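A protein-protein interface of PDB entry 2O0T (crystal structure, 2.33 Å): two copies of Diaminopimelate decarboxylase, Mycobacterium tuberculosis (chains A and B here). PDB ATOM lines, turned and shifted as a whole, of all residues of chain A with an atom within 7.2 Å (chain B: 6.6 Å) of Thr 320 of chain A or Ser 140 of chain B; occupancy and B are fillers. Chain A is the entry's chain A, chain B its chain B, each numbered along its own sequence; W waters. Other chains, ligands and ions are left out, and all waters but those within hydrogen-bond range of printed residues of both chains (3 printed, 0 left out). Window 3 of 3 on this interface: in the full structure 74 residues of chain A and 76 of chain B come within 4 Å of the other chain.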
ATOM      1  N   GLU A 317     -18.304 -16.541  -9.168  1.00  0.00           N
ATOM      2  CA  GLU A 317     -18.391 -15.564  -8.057  1.00  0.00           C
ATOM      3  C   GLU A 317     -19.299 -16.116  -6.928  1.00  0.00           C
ATOM      4  O   GLU A 317     -20.424 -16.512  -7.197  1.00  0.00           O
ATOM      5  CB  GLU A 317     -18.930 -14.186  -8.528  1.00  0.00           C
ATOM      6  CG  GLU A 317     -18.820 -13.085  -7.398  1.00  0.00           C
ATOM      7  CD  GLU A 317     -19.373 -11.668  -7.744  1.00  0.00           C
ATOM      8  OE1 GLU A 317     -19.588 -11.299  -8.912  1.00  0.00           O
ATOM      9  OE2 GLU A 317     -19.601 -10.879  -6.813  1.00  0.00           O
ATOM     10  N   VAL A 318     -18.791 -16.118  -5.683  1.00  0.00           N
ATOM     11  CA  VAL A 318     -19.621 -16.406  -4.510  1.00  0.00           C
ATOM     12  C   VAL A 318     -20.653 -15.316  -4.275  1.00  0.00           C
ATOM     13  O   VAL A 318     -20.312 -14.139  -4.121  1.00  0.00           O
ATOM     14  CB  VAL A 318     -18.782 -16.659  -3.199  1.00  0.00           C
ATOM     15  CG1 VAL A 318     -19.679 -16.750  -1.942  1.00  0.00           C
ATOM     16  CG2 VAL A 318     -17.924 -17.920  -3.345  1.00  0.00           C
ATOM     17  N   GLY A 319     -21.933 -15.732  -4.252  1.00  0.00           N
ATOM     18  CA  GLY A 319     -23.087 -14.844  -3.995  1.00  0.00           C
ATOM     19  C   GLY A 319     -23.644 -14.906  -2.584  1.00  0.00           C
ATOM     20  O   GLY A 319     -24.033 -13.866  -2.024  1.00  0.00           O
ATOM     21  N   THR A 320     -23.730 -16.120  -2.034  1.00  0.00           N
ATOM     22  CA  THR A 320     -24.316 -16.380  -0.718  1.00  0.00           C
ATOM     23  C   THR A 320     -23.557 -17.469   0.003  1.00  0.00           C
ATOM     24  O   THR A 320     -23.149 -18.489  -0.588  1.00  0.00           O
ATOM     25  CB  THR A 320     -25.824 -16.881  -0.774  1.00  0.00           C
ATOM     26  OG1 THR A 320     -26.602 -15.998  -1.562  1.00  0.00           O
ATOM     27  CG2 THR A 320     -26.492 -16.978   0.669  1.00  0.00           C
ATOM     28  N   VAL A 321     -23.460 -17.286   1.302  1.00  0.00           N
ATOM     29  CA  VAL A 321     -22.842 -18.200   2.189  1.00  0.00           C
ATOM     30  C   VAL A 321     -23.845 -18.418   3.329  1.00  0.00           C
ATOM     31  O   VAL A 321     -24.198 -17.487   4.071  1.00  0.00           O
ATOM     32  CB  VAL A 321     -21.476 -17.621   2.742  1.00  0.00           C
ATOM     33  CG1 VAL A 321     -20.826 -18.597   3.701  1.00  0.00           C
ATOM     34  CG2 VAL A 321     -20.495 -17.219   1.595  1.00  0.00           C
ATOM     35  N   LYS A 322     -24.305 -19.670   3.458  1.00  0.00           N
ATOM     36  CA  LYS A 322     -25.231 -20.053   4.498  1.00  0.00           C
ATOM     37  C   LYS A 322     -24.687 -21.237   5.320  1.00  0.00           C
ATOM     38  O   LYS A 322     -24.325 -22.304   4.765  1.00  0.00           O
ATOM     39  CB  LYS A 322     -26.598 -20.431   3.864  1.00  0.00           C
ATOM     40  CG  LYS A 322     -27.727 -20.747   4.935  1.00  0.00           C
ATOM     41  CD  LYS A 322     -29.024 -21.256   4.360  1.00  0.00           C
ATOM     42  CE  LYS A 322     -29.735 -20.248   3.433  1.00  0.00           C
ATOM     43  NZ  LYS A 322     -31.029 -20.780   2.898  1.00  0.00           N
ATOM     44  N   TYR A 334     -22.894 -23.861   3.107  1.00  0.00           N
ATOM     45  CA  TYR A 334     -23.374 -23.824   1.738  1.00  0.00           C
ATOM     46  C   TYR A 334     -22.935 -22.533   1.050  1.00  0.00           C
ATOM     47  O   TYR A 334     -23.312 -21.390   1.434  1.00  0.00           O
ATOM     48  CB  TYR A 334     -24.896 -24.011   1.687  1.00  0.00           C
ATOM     49  CG  TYR A 334     -25.369 -25.435   1.805  1.00  0.00           C
ATOM     50  CD1 TYR A 334     -25.245 -26.140   3.014  1.00  0.00           C
ATOM     51  CD2 TYR A 334     -25.992 -26.052   0.731  1.00  0.00           C
ATOM     52  CE1 TYR A 334     -25.683 -27.441   3.112  1.00  0.00           C
ATOM     53  CE2 TYR A 334     -26.454 -27.346   0.800  1.00  0.00           C
ATOM     54  CZ  TYR A 334     -26.305 -28.035   1.991  1.00  0.00           C
ATOM     55  OH  TYR A 334     -26.740 -29.313   2.059  1.00  0.00           O
ATOM     56  N   VAL A 335     -22.126 -22.725   0.023  1.00  0.00           N
ATOM     57  CA  VAL A 335     -21.657 -21.610  -0.772  1.00  0.00           C
ATOM     58  C   VAL A 335     -22.281 -21.591  -2.159  1.00  0.00           C
ATOM     59  O   VAL A 335     -22.108 -22.517  -2.951  1.00  0.00           O
ATOM     60  CB  VAL A 335     -20.113 -21.319  -0.647  1.00  0.00           C
ATOM     61  CG1 VAL A 335     -19.404 -22.198   0.414  1.00  0.00           C
ATOM     62  CG2 VAL A 335     -19.419 -21.195  -1.985  1.00  0.00           C
ATOM     63  N   SER A 336     -23.148 -20.590  -2.339  1.00  0.00           N
ATOM     64  CA  SER A 336     -23.917 -20.385  -3.559  1.00  0.00           C
ATOM     65  C   SER A 336     -23.121 -19.508  -4.537  1.00  0.00           C
ATOM     66  O   SER A 336     -22.478 -18.491  -4.226  1.00  0.00           O
ATOM     67  CB  SER A 336     -25.298 -19.740  -3.345  1.00  0.00           C
ATOM     68  OG  SER A 336     -26.104 -20.479  -2.471  1.00  0.00           O
ATOM     69  N   VAL A 337     -23.249 -19.917  -5.754  1.00  0.00           N
ATOM     70  CA  VAL A 337     -22.410 -19.459  -6.753  1.00  0.00           C
ATOM     71  C   VAL A 337     -23.314 -19.161  -7.949  1.00  0.00           C
ATOM     72  O   VAL A 337     -24.548 -19.402  -8.000  1.00  0.00           O
ATOM     73  CB  VAL A 337     -21.264 -20.534  -7.002  1.00  0.00           C
ATOM     74  CG1 VAL A 337     -21.369 -21.265  -8.363  1.00  0.00           C
ATOM     75  CG2 VAL A 337     -19.862 -19.990  -6.611  1.00  0.00           C
ATOM     76  N   VAL A 373     -22.982 -25.088  -4.383  1.00  0.00           N
ATOM     77  CA  VAL A 373     -24.327 -25.177  -4.988  1.00  0.00           C
ATOM     78  C   VAL A 373     -24.522 -23.969  -5.939  1.00  0.00           C
ATOM     79  O   VAL A 373     -23.869 -22.895  -5.791  1.00  0.00           O
ATOM     80  CB  VAL A 373     -25.502 -25.202  -3.887  1.00  0.00           C
ATOM     81  CG1 VAL A 373     -25.474 -26.484  -2.999  1.00  0.00           C
ATOM     82  CG2 VAL A 373     -25.503 -23.903  -2.980  1.00  0.00           C
ATOM     83  N   ILE A 393     -14.820 -17.494   3.869  1.00  0.00           N
ATOM     84  CA  ILE A 393     -15.359 -17.318   2.528  1.00  0.00           C
ATOM     85  C   ILE A 393     -16.575 -16.388   2.574  1.00  0.00           C
ATOM     86  O   ILE A 393     -17.416 -16.477   3.484  1.00  0.00           O
ATOM     87  CB  ILE A 393     -15.744 -18.667   1.865  1.00  0.00           C
ATOM     88  CG1 ILE A 393     -15.903 -18.490   0.366  1.00  0.00           C
ATOM     89  CG2 ILE A 393     -16.972 -19.205   2.468  1.00  0.00           C
ATOM     90  CD1 ILE A 393     -15.391 -19.631  -0.381  1.00  0.00           C
ATOM     91  N   ARG A 394     -16.660 -15.514   1.580  1.00  0.00           N
ATOM     92  CA  ARG A 394     -17.528 -14.351   1.621  1.00  0.00           C
ATOM     93  C   ARG A 394     -18.060 -14.093   0.214  1.00  0.00           C
ATOM     94  O   ARG A 394     -17.418 -14.512  -0.780  1.00  0.00           O
ATOM     95  CB  ARG A 394     -16.755 -13.103   2.158  1.00  0.00           C
ATOM     96  CG  ARG A 394     -15.425 -12.808   1.378  1.00  0.00           C
ATOM     97  CD  ARG A 394     -14.792 -11.389   1.605  1.00  0.00           C
ATOM     98  NE  ARG A 394     -14.266 -11.339   2.952  1.00  0.00           N
ATOM     99  CZ  ARG A 394     -12.992 -11.123   3.265  1.00  0.00           C
ATOM    100  NH1 ARG A 394     -12.661 -11.122   4.559  1.00  0.00           N
ATOM    101  NH2 ARG A 394     -12.069 -10.880   2.316  1.00  0.00           N
ATOM    102  N   PRO A 395     -19.250 -13.430   0.104  1.00  0.00           N
ATOM    103  CA  PRO A 395     -19.732 -13.059  -1.231  1.00  0.00           C
ATOM    104  C   PRO A 395     -18.705 -12.131  -1.863  1.00  0.00           C
ATOM    105  O   PRO A 395     -18.107 -11.289  -1.148  1.00  0.00           O
ATOM    106  CB  PRO A 395     -21.017 -12.308  -0.944  1.00  0.00           C
ATOM    107  CG  PRO A 395     -21.461 -12.884   0.323  1.00  0.00           C
ATOM    108  CD  PRO A 395     -20.189 -12.963   1.134  1.00  0.00           C
ATOM    109  N   GLY A 396     -18.480 -12.316  -3.158  1.00  0.00           N
ATOM    110  CA  GLY A 396     -17.503 -11.545  -3.898  1.00  0.00           C
ATOM    111  C   GLY A 396     -16.171 -12.265  -4.061  1.00  0.00           C
ATOM    112  O   GLY A 396     -15.378 -11.907  -4.919  1.00  0.00           O
ATOM    113  N   GLY B 117     -35.524 -18.010  -5.160  1.00  0.00           N
ATOM    114  CA  GLY B 117     -34.118 -18.436  -5.392  1.00  0.00           C
ATOM    115  C   GLY B 117     -33.227 -18.318  -4.178  1.00  0.00           C
ATOM    116  O   GLY B 117     -33.387 -17.382  -3.322  1.00  0.00           O
ATOM    117  N   ASN B 118     -32.253 -19.219  -4.142  1.00  0.00           N
ATOM    118  CA  ASN B 118     -31.306 -19.269  -3.022  1.00  0.00           C
ATOM    119  C   ASN B 118     -30.122 -18.296  -3.138  1.00  0.00           C
ATOM    120  O   ASN B 118     -29.417 -18.052  -2.145  1.00  0.00           O
ATOM    121  CB  ASN B 118     -30.753 -20.676  -2.845  1.00  0.00           C
ATOM    122  CG  ASN B 118     -29.850 -21.106  -3.990  1.00  0.00           C
ATOM    123  OD1 ASN B 118     -28.604 -21.225  -3.847  1.00  0.00           O
ATOM    124  ND2 ASN B 118     -30.467 -21.408  -5.111  1.00  0.00           N
ATOM    125  N   ASN B 119     -29.889 -17.797  -4.358  1.00  0.00           N
ATOM    126  CA  ASN B 119     -28.749 -16.942  -4.639  1.00  0.00           C
ATOM    127  C   ASN B 119     -29.104 -15.726  -5.546  1.00  0.00           C
ATOM    128  O   ASN B 119     -28.416 -15.453  -6.539  1.00  0.00           O
ATOM    129  CB  ASN B 119     -27.590 -17.750  -5.241  1.00  0.00           C
ATOM    130  CG  ASN B 119     -26.304 -16.964  -5.261  1.00  0.00           C
ATOM    131  OD1 ASN B 119     -25.411 -17.238  -6.070  1.00  0.00           O
ATOM    132  ND2 ASN B 119     -26.199 -15.952  -4.371  1.00  0.00           N
ATOM    133  N   LYS B 120     -30.149 -14.977  -5.187  1.00  0.00           N
ATOM    134  CA  LYS B 120     -30.535 -13.800  -5.966  1.00  0.00           C
ATOM    135  C   LYS B 120     -29.413 -12.743  -5.869  1.00  0.00           C
ATOM    136  O   LYS B 120     -28.954 -12.408  -4.772  1.00  0.00           O
ATOM    137  CB  LYS B 120     -31.857 -13.218  -5.450  1.00  0.00           C
ATOM    138  CG  LYS B 120     -32.955 -14.253  -5.279  1.00  0.00           C
ATOM    139  CD  LYS B 120     -34.301 -13.551  -5.079  1.00  0.00           C
ATOM    140  CE  LYS B 120     -35.398 -14.493  -4.630  1.00  0.00           C
ATOM    141  NZ  LYS B 120     -35.177 -15.139  -3.272  1.00  0.00           N
ATOM    142  N   VAL B 137     -39.659 -14.040  -2.293  1.00  0.00           N
ATOM    143  CA  VAL B 137     -39.449 -15.035  -1.249  1.00  0.00           C
ATOM    144  C   VAL B 137     -37.980 -15.068  -0.876  1.00  0.00           C
ATOM    145  O   VAL B 137     -37.147 -15.604  -1.604  1.00  0.00           O
ATOM    146  CB  VAL B 137     -39.956 -16.419  -1.701  1.00  0.00           C
ATOM    147  CG1 VAL B 137     -39.802 -17.475  -0.558  1.00  0.00           C
ATOM    148  CG2 VAL B 137     -41.443 -16.296  -2.063  1.00  0.00           C
ATOM    149  N   VAL B 138     -37.675 -14.468   0.263  1.00  0.00           N
ATOM    150  CA  VAL B 138     -36.306 -14.358   0.742  1.00  0.00           C
ATOM    151  C   VAL B 138     -35.740 -15.693   1.324  1.00  0.00           C
ATOM    152  O   VAL B 138     -36.453 -16.429   1.991  1.00  0.00           O
ATOM    153  CB  VAL B 138     -36.202 -13.134   1.717  1.00  0.00           C
ATOM    154  CG1 VAL B 138     -36.794 -11.963   1.035  1.00  0.00           C
ATOM    155  CG2 VAL B 138     -36.907 -13.398   3.089  1.00  0.00           C
ATOM    156  N   ASP B 139     -34.478 -15.996   1.015  1.00  0.00           N
ATOM    157  CA  ASP B 139     -33.889 -17.287   1.348  1.00  0.00           C
ATOM    158  C   ASP B 139     -32.702 -17.251   2.318  1.00  0.00           C
ATOM    159  O   ASP B 139     -32.238 -18.321   2.693  1.00  0.00           O
ATOM    160  CB  ASP B 139     -33.377 -17.955   0.062  1.00  0.00           C
ATOM    161  CG  ASP B 139     -33.259 -19.482   0.195  1.00  0.00           C
ATOM    162  OD1 ASP B 139     -34.322 -20.114   0.337  1.00  0.00           O
ATOM    163  OD2 ASP B 139     -32.135 -20.055   0.151  1.00  0.00           O
ATOM    164  N   SER B 140     -32.201 -16.058   2.687  1.00  0.00           N
ATOM    165  CA  SER B 140     -31.023 -15.915   3.521  1.00  0.00           C
ATOM    166  C   SER B 140     -31.015 -14.521   4.177  1.00  0.00           C
ATOM    167  O   SER B 140     -31.723 -13.589   3.743  1.00  0.00           O
ATOM    168  CB  SER B 140     -29.765 -16.046   2.685  1.00  0.00           C
ATOM    169  OG  SER B 140     -29.673 -14.935   1.793  1.00  0.00           O
ATOM    170  N   MET B 141     -30.232 -14.411   5.253  1.00  0.00           N
ATOM    171  CA  MET B 141     -30.050 -13.170   5.936  1.00  0.00           C
ATOM    172  C   MET B 141     -29.446 -12.115   5.002  1.00  0.00           C
ATOM    173  O   MET B 141     -29.855 -10.956   5.025  1.00  0.00           O
ATOM    174  CB  MET B 141     -29.174 -13.409   7.134  1.00  0.00           C
ATOM    175  CG  MET B 141     -29.923 -14.107   8.262  1.00  0.00           C
ATOM    176  SD  MET B 141     -31.417 -13.217   8.871  1.00  0.00           S
ATOM    177  CE  MET B 141     -30.782 -11.598   9.295  1.00  0.00           C
ATOM    178  N   THR B 142     -28.496 -12.546   4.181  1.00  0.00           N
ATOM    179  CA  THR B 142     -27.839 -11.694   3.188  1.00  0.00           C
ATOM    180  C   THR B 142     -28.835 -11.086   2.195  1.00  0.00           C
ATOM    181  O   THR B 142     -28.766  -9.905   1.891  1.00  0.00           O
ATOM    182  CB  THR B 142     -26.762 -12.492   2.351  1.00  0.00           C
ATOM    183  OG1 THR B 142     -25.929 -13.259   3.232  1.00  0.00           O
ATOM    184  CG2 THR B 142     -25.900 -11.546   1.542  1.00  0.00           C
ATOM    185  N   GLU B 143     -29.731 -11.907   1.652  1.00  0.00           N
ATOM    186  CA  GLU B 143     -30.747 -11.414   0.734  1.00  0.00           C
ATOM    187  C   GLU B 143     -31.595 -10.324   1.423  1.00  0.00           C
ATOM    188  O   GLU B 143     -31.874  -9.264   0.855  1.00  0.00           O
ATOM    189  CB  GLU B 143     -31.659 -12.546   0.260  1.00  0.00           C
ATOM    190  CG  GLU B 143     -32.675 -12.060  -0.841  1.00  0.00           C
ATOM    191  CD  GLU B 143     -33.618 -13.139  -1.296  1.00  0.00           C
ATOM    192  OE1 GLU B 143     -33.252 -14.336  -1.191  1.00  0.00           O
ATOM    193  OE2 GLU B 143     -34.730 -12.812  -1.778  1.00  0.00           O
ATOM    194  N   ILE B 144     -31.998 -10.586   2.658  1.00  0.00           N
ATOM    195  CA  ILE B 144     -32.770  -9.608   3.411  1.00  0.00           C
ATOM    196  C   ILE B 144     -32.056  -8.242   3.494  1.00  0.00           C
ATOM    197  O   ILE B 144     -32.660  -7.219   3.157  1.00  0.00           O
ATOM    198  CB  ILE B 144     -33.101 -10.163   4.795  1.00  0.00           C
ATOM    199  CG1 ILE B 144     -34.083 -11.330   4.649  1.00  0.00           C
ATOM    200  CG2 ILE B 144     -33.664  -9.083   5.711  1.00  0.00           C
ATOM    201  CD1 ILE B 144     -34.192 -12.126   5.947  1.00  0.00           C
ATOM    202  N   GLU B 145     -30.775  -8.234   3.867  1.00  0.00           N
ATOM    203  CA  GLU B 145     -29.978  -7.003   3.902  1.00  0.00           C
ATOM    204  C   GLU B 145     -29.851  -6.332   2.518  1.00  0.00           C
ATOM    205  O   GLU B 145     -29.978  -5.108   2.407  1.00  0.00           O
ATOM    206  CB  GLU B 145     -28.595  -7.310   4.448  1.00  0.00           C
ATOM    207  CG  GLU B 145     -28.680  -7.960   5.809  1.00  0.00           C
ATOM    208  CD  GLU B 145     -27.403  -8.681   6.225  1.00  0.00           C
ATOM    209  OE1 GLU B 145     -26.647  -9.180   5.364  1.00  0.00           O
ATOM    210  OE2 GLU B 145     -27.169  -8.752   7.434  1.00  0.00           O
ATOM    211  N   ARG B 146     -29.630  -7.130   1.468  1.00  0.00           N
ATOM    212  CA  ARG B 146     -29.575  -6.564   0.140  1.00  0.00           C
ATOM    213  C   ARG B 146     -30.880  -5.903  -0.231  1.00  0.00           C
ATOM    214  O   ARG B 146     -30.858  -4.778  -0.715  1.00  0.00           O
ATOM    215  CB  ARG B 146     -29.231  -7.595  -0.942  1.00  0.00           C
ATOM    216  CG  ARG B 146     -27.808  -8.036  -0.899  1.00  0.00           C
ATOM    217  CD  ARG B 146     -27.670  -9.428  -1.565  1.00  0.00           C
ATOM    218  NE  ARG B 146     -26.254  -9.722  -1.657  1.00  0.00           N
ATOM    219  CZ  ARG B 146     -25.707 -10.928  -1.843  1.00  0.00           C
ATOM    220  NH1 ARG B 146     -24.373 -10.997  -1.877  1.00  0.00           N
ATOM    221  NH2 ARG B 146     -26.471 -12.053  -1.969  1.00  0.00           N
ATOM    222  N   GLY B 186     -33.947 -21.943   2.257  1.00  0.00           N
ATOM    223  CA  GLY B 186     -34.707 -21.634   3.461  1.00  0.00           C
ATOM    224  C   GLY B 186     -33.894 -21.527   4.727  1.00  0.00           C
ATOM    225  O   GLY B 186     -32.653 -21.713   4.741  1.00  0.00           O
ATOM    226  N   LEU B 187     -34.616 -21.200   5.800  1.00  0.00           N
ATOM    227  CA  LEU B 187     -34.058 -21.046   7.149  1.00  0.00           C
ATOM    228  C   LEU B 187     -34.815 -21.949   8.086  1.00  0.00           C
ATOM    229  O   LEU B 187     -36.050 -22.075   8.003  1.00  0.00           O
ATOM    230  CB  LEU B 187     -34.210 -19.584   7.592  1.00  0.00           C
ATOM    231  CG  LEU B 187     -33.507 -18.665   6.564  1.00  0.00           C
ATOM    232  CD1 LEU B 187     -34.330 -17.466   6.063  1.00  0.00           C
ATOM    233  CD2 LEU B 187     -32.078 -18.276   6.993  1.00  0.00           C
ATOM    234  N   ALA B 197     -34.619 -14.256  11.066  1.00  0.00           N
ATOM    235  CA  ALA B 197     -34.901 -13.625   9.783  1.00  0.00           C
ATOM    236  C   ALA B 197     -36.158 -12.778   9.878  1.00  0.00           C
ATOM    237  O   ALA B 197     -36.166 -11.661   9.384  1.00  0.00           O
ATOM    238  CB  ALA B 197     -35.019 -14.661   8.641  1.00  0.00           C
HETATM  239  O   HOH W   1     -23.034 -15.833  -7.051  1.00  0.00           O
HETATM  240  O   HOH W   2     -26.261 -13.307  -4.612  1.00  0.00           O
HETATM  241  O   HOH W   3     -23.906 -14.496   2.313  1.00  0.00           O
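NZ of Lys 322 of chain A lies within hydrogen-bond range of O of Gly 186 of chain B (2.6 Å).
The side-chain amide nitrogen of Asn 119 of chain B lies within hydrogen-bond range of the side-chain hydroxyl of Thr 320 of chain A (2.8 Å).
O of Gly 319 of chain A lies within hydrogen-bond range of NH1 of Arg 146 of chain B.
The side-chain amide oxygen (OD1) of Asn 119 of chain B lies close to the backbone carbonyl oxygen (O) of Val 337 of chain A (3.0 Å).
The side-chain amino group (NZ) of Lys 322 of chain A lies within salt-bridge range of the side-chain carboxylate (OD2) of Asp 139 of chain B (3.0 Å).
OG of Ser 336 of chain A is in hydrogen-bond range of OD1 of Asn 118 of chain B (2.9 Å).
Water W3 lies within hydrogen-bond range of the side-chain hydroxyl (OG1) of Thr 142 of chain B and the backbone NH (N) of Val 321 of chain A.
Water W2 lies within hydrogen-bond range of ND2 of Asn 119 of chain B (2.7 Å), O of Lys 120 of chain B (2.8 Å), NH2 of Arg 146 of chain B (2.9 Å) and O of Gly 319 of chain A (3.5 Å).
Water W1 lies within hydrogen-bond range of the backbone carbonyl oxygen of Glu 317 of chain A, the side-chain amide oxygen of Asn 119 of chain B and the backbone NH of Gly 319 of chain A.
Of the printed residues of chain B, Gly 319 of chain A touches Asn 119 and Arg 146.
Thr 320 of chain A touches just these residues of chain B: Asn 118 (3.5 Å), Asn 119 (2.8 Å), Ser 140 (3.9 Å) and Arg 146 (3.97 Å).
Of the printed residues of chain B, Lys 322 of chain A touches Asp 139 and Gly 186.
Of the printed residues of chain B, Val 337 of chain A touches Asn 119 (3.0 Å).
Of chain A, only Thr 320 comes within 4 Å of Ser 140 of chain B.
The nearest residue of chain A that does not touch Ser 140 of chain B is Lys 322 of chain A (4.3 Å).
The nearest printed residue of chain B that does not touch Ser 336 of chain A is Asp 139 of chain B (6.6 Å).
No position is printed for both chains.
Of the 12 pairs that touch across the chains among the printed residues, none has its exchanged pair printed and touching as well.
Printed residues of chain A that touch a printed residue of chain B: Gly 319, Thr 320, Lys 322, Ser 336, Val 337 and Pro 395.
Hydrophobic or aromatic side chains of chain A that line the printed part of chain B: Pro 395.
Among the printed residues, Asp or Glu carboxylates within 4 Å of a Lys or Arg side-chain nitrogen of the other chain: Lys 322 of chain A with Asp 139 of chain B.
N of Tyr 334 of chain A sits at hydrogen-bond distance from O of Lys 322 of chain A (2.7 Å).
O of Val 373 of chain A is in hydrogen-bond range of N of Val 337 of chain A (3.0 Å).
The backbone NH of Gly 186 of chain B is in hydrogen-bond range of the side-chain carboxylate of Asp 139 of chain B (2.7 Å).
O of Thr 320 of chain A lies within hydrogen-bond range of N of Ser 336 of chain A, 2.7 Å away.
The side-chain hydroxyl of Ser 140 of chain B is in hydrogen-bond range of the backbone NH of Glu 143 of chain B (3.0 Å).
The backbone carbonyl oxygen (O) of Ser 336 of chain A sits at hydrogen-bond distance from the backbone NH (N) of Gly 319 of chain A (2.8 Å).
Among the printed residues, merely in contact across the chains: Gly 319 of chain A with Asn 119 of chain B (3.3 Å), Ser 336 of chain A with Asn 119 of chain B (3.5 Å), Thr 320 of chain A with Asn 118 of chain B (3.5 Å), Pro 395 of chain A with Arg 146 of chain B (3.7 Å), Thr 320 of chain A with Ser 140 of chain B (3.9 Å) and Thr 320 of chain A with Arg 146 of chain B (3.97 Å).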
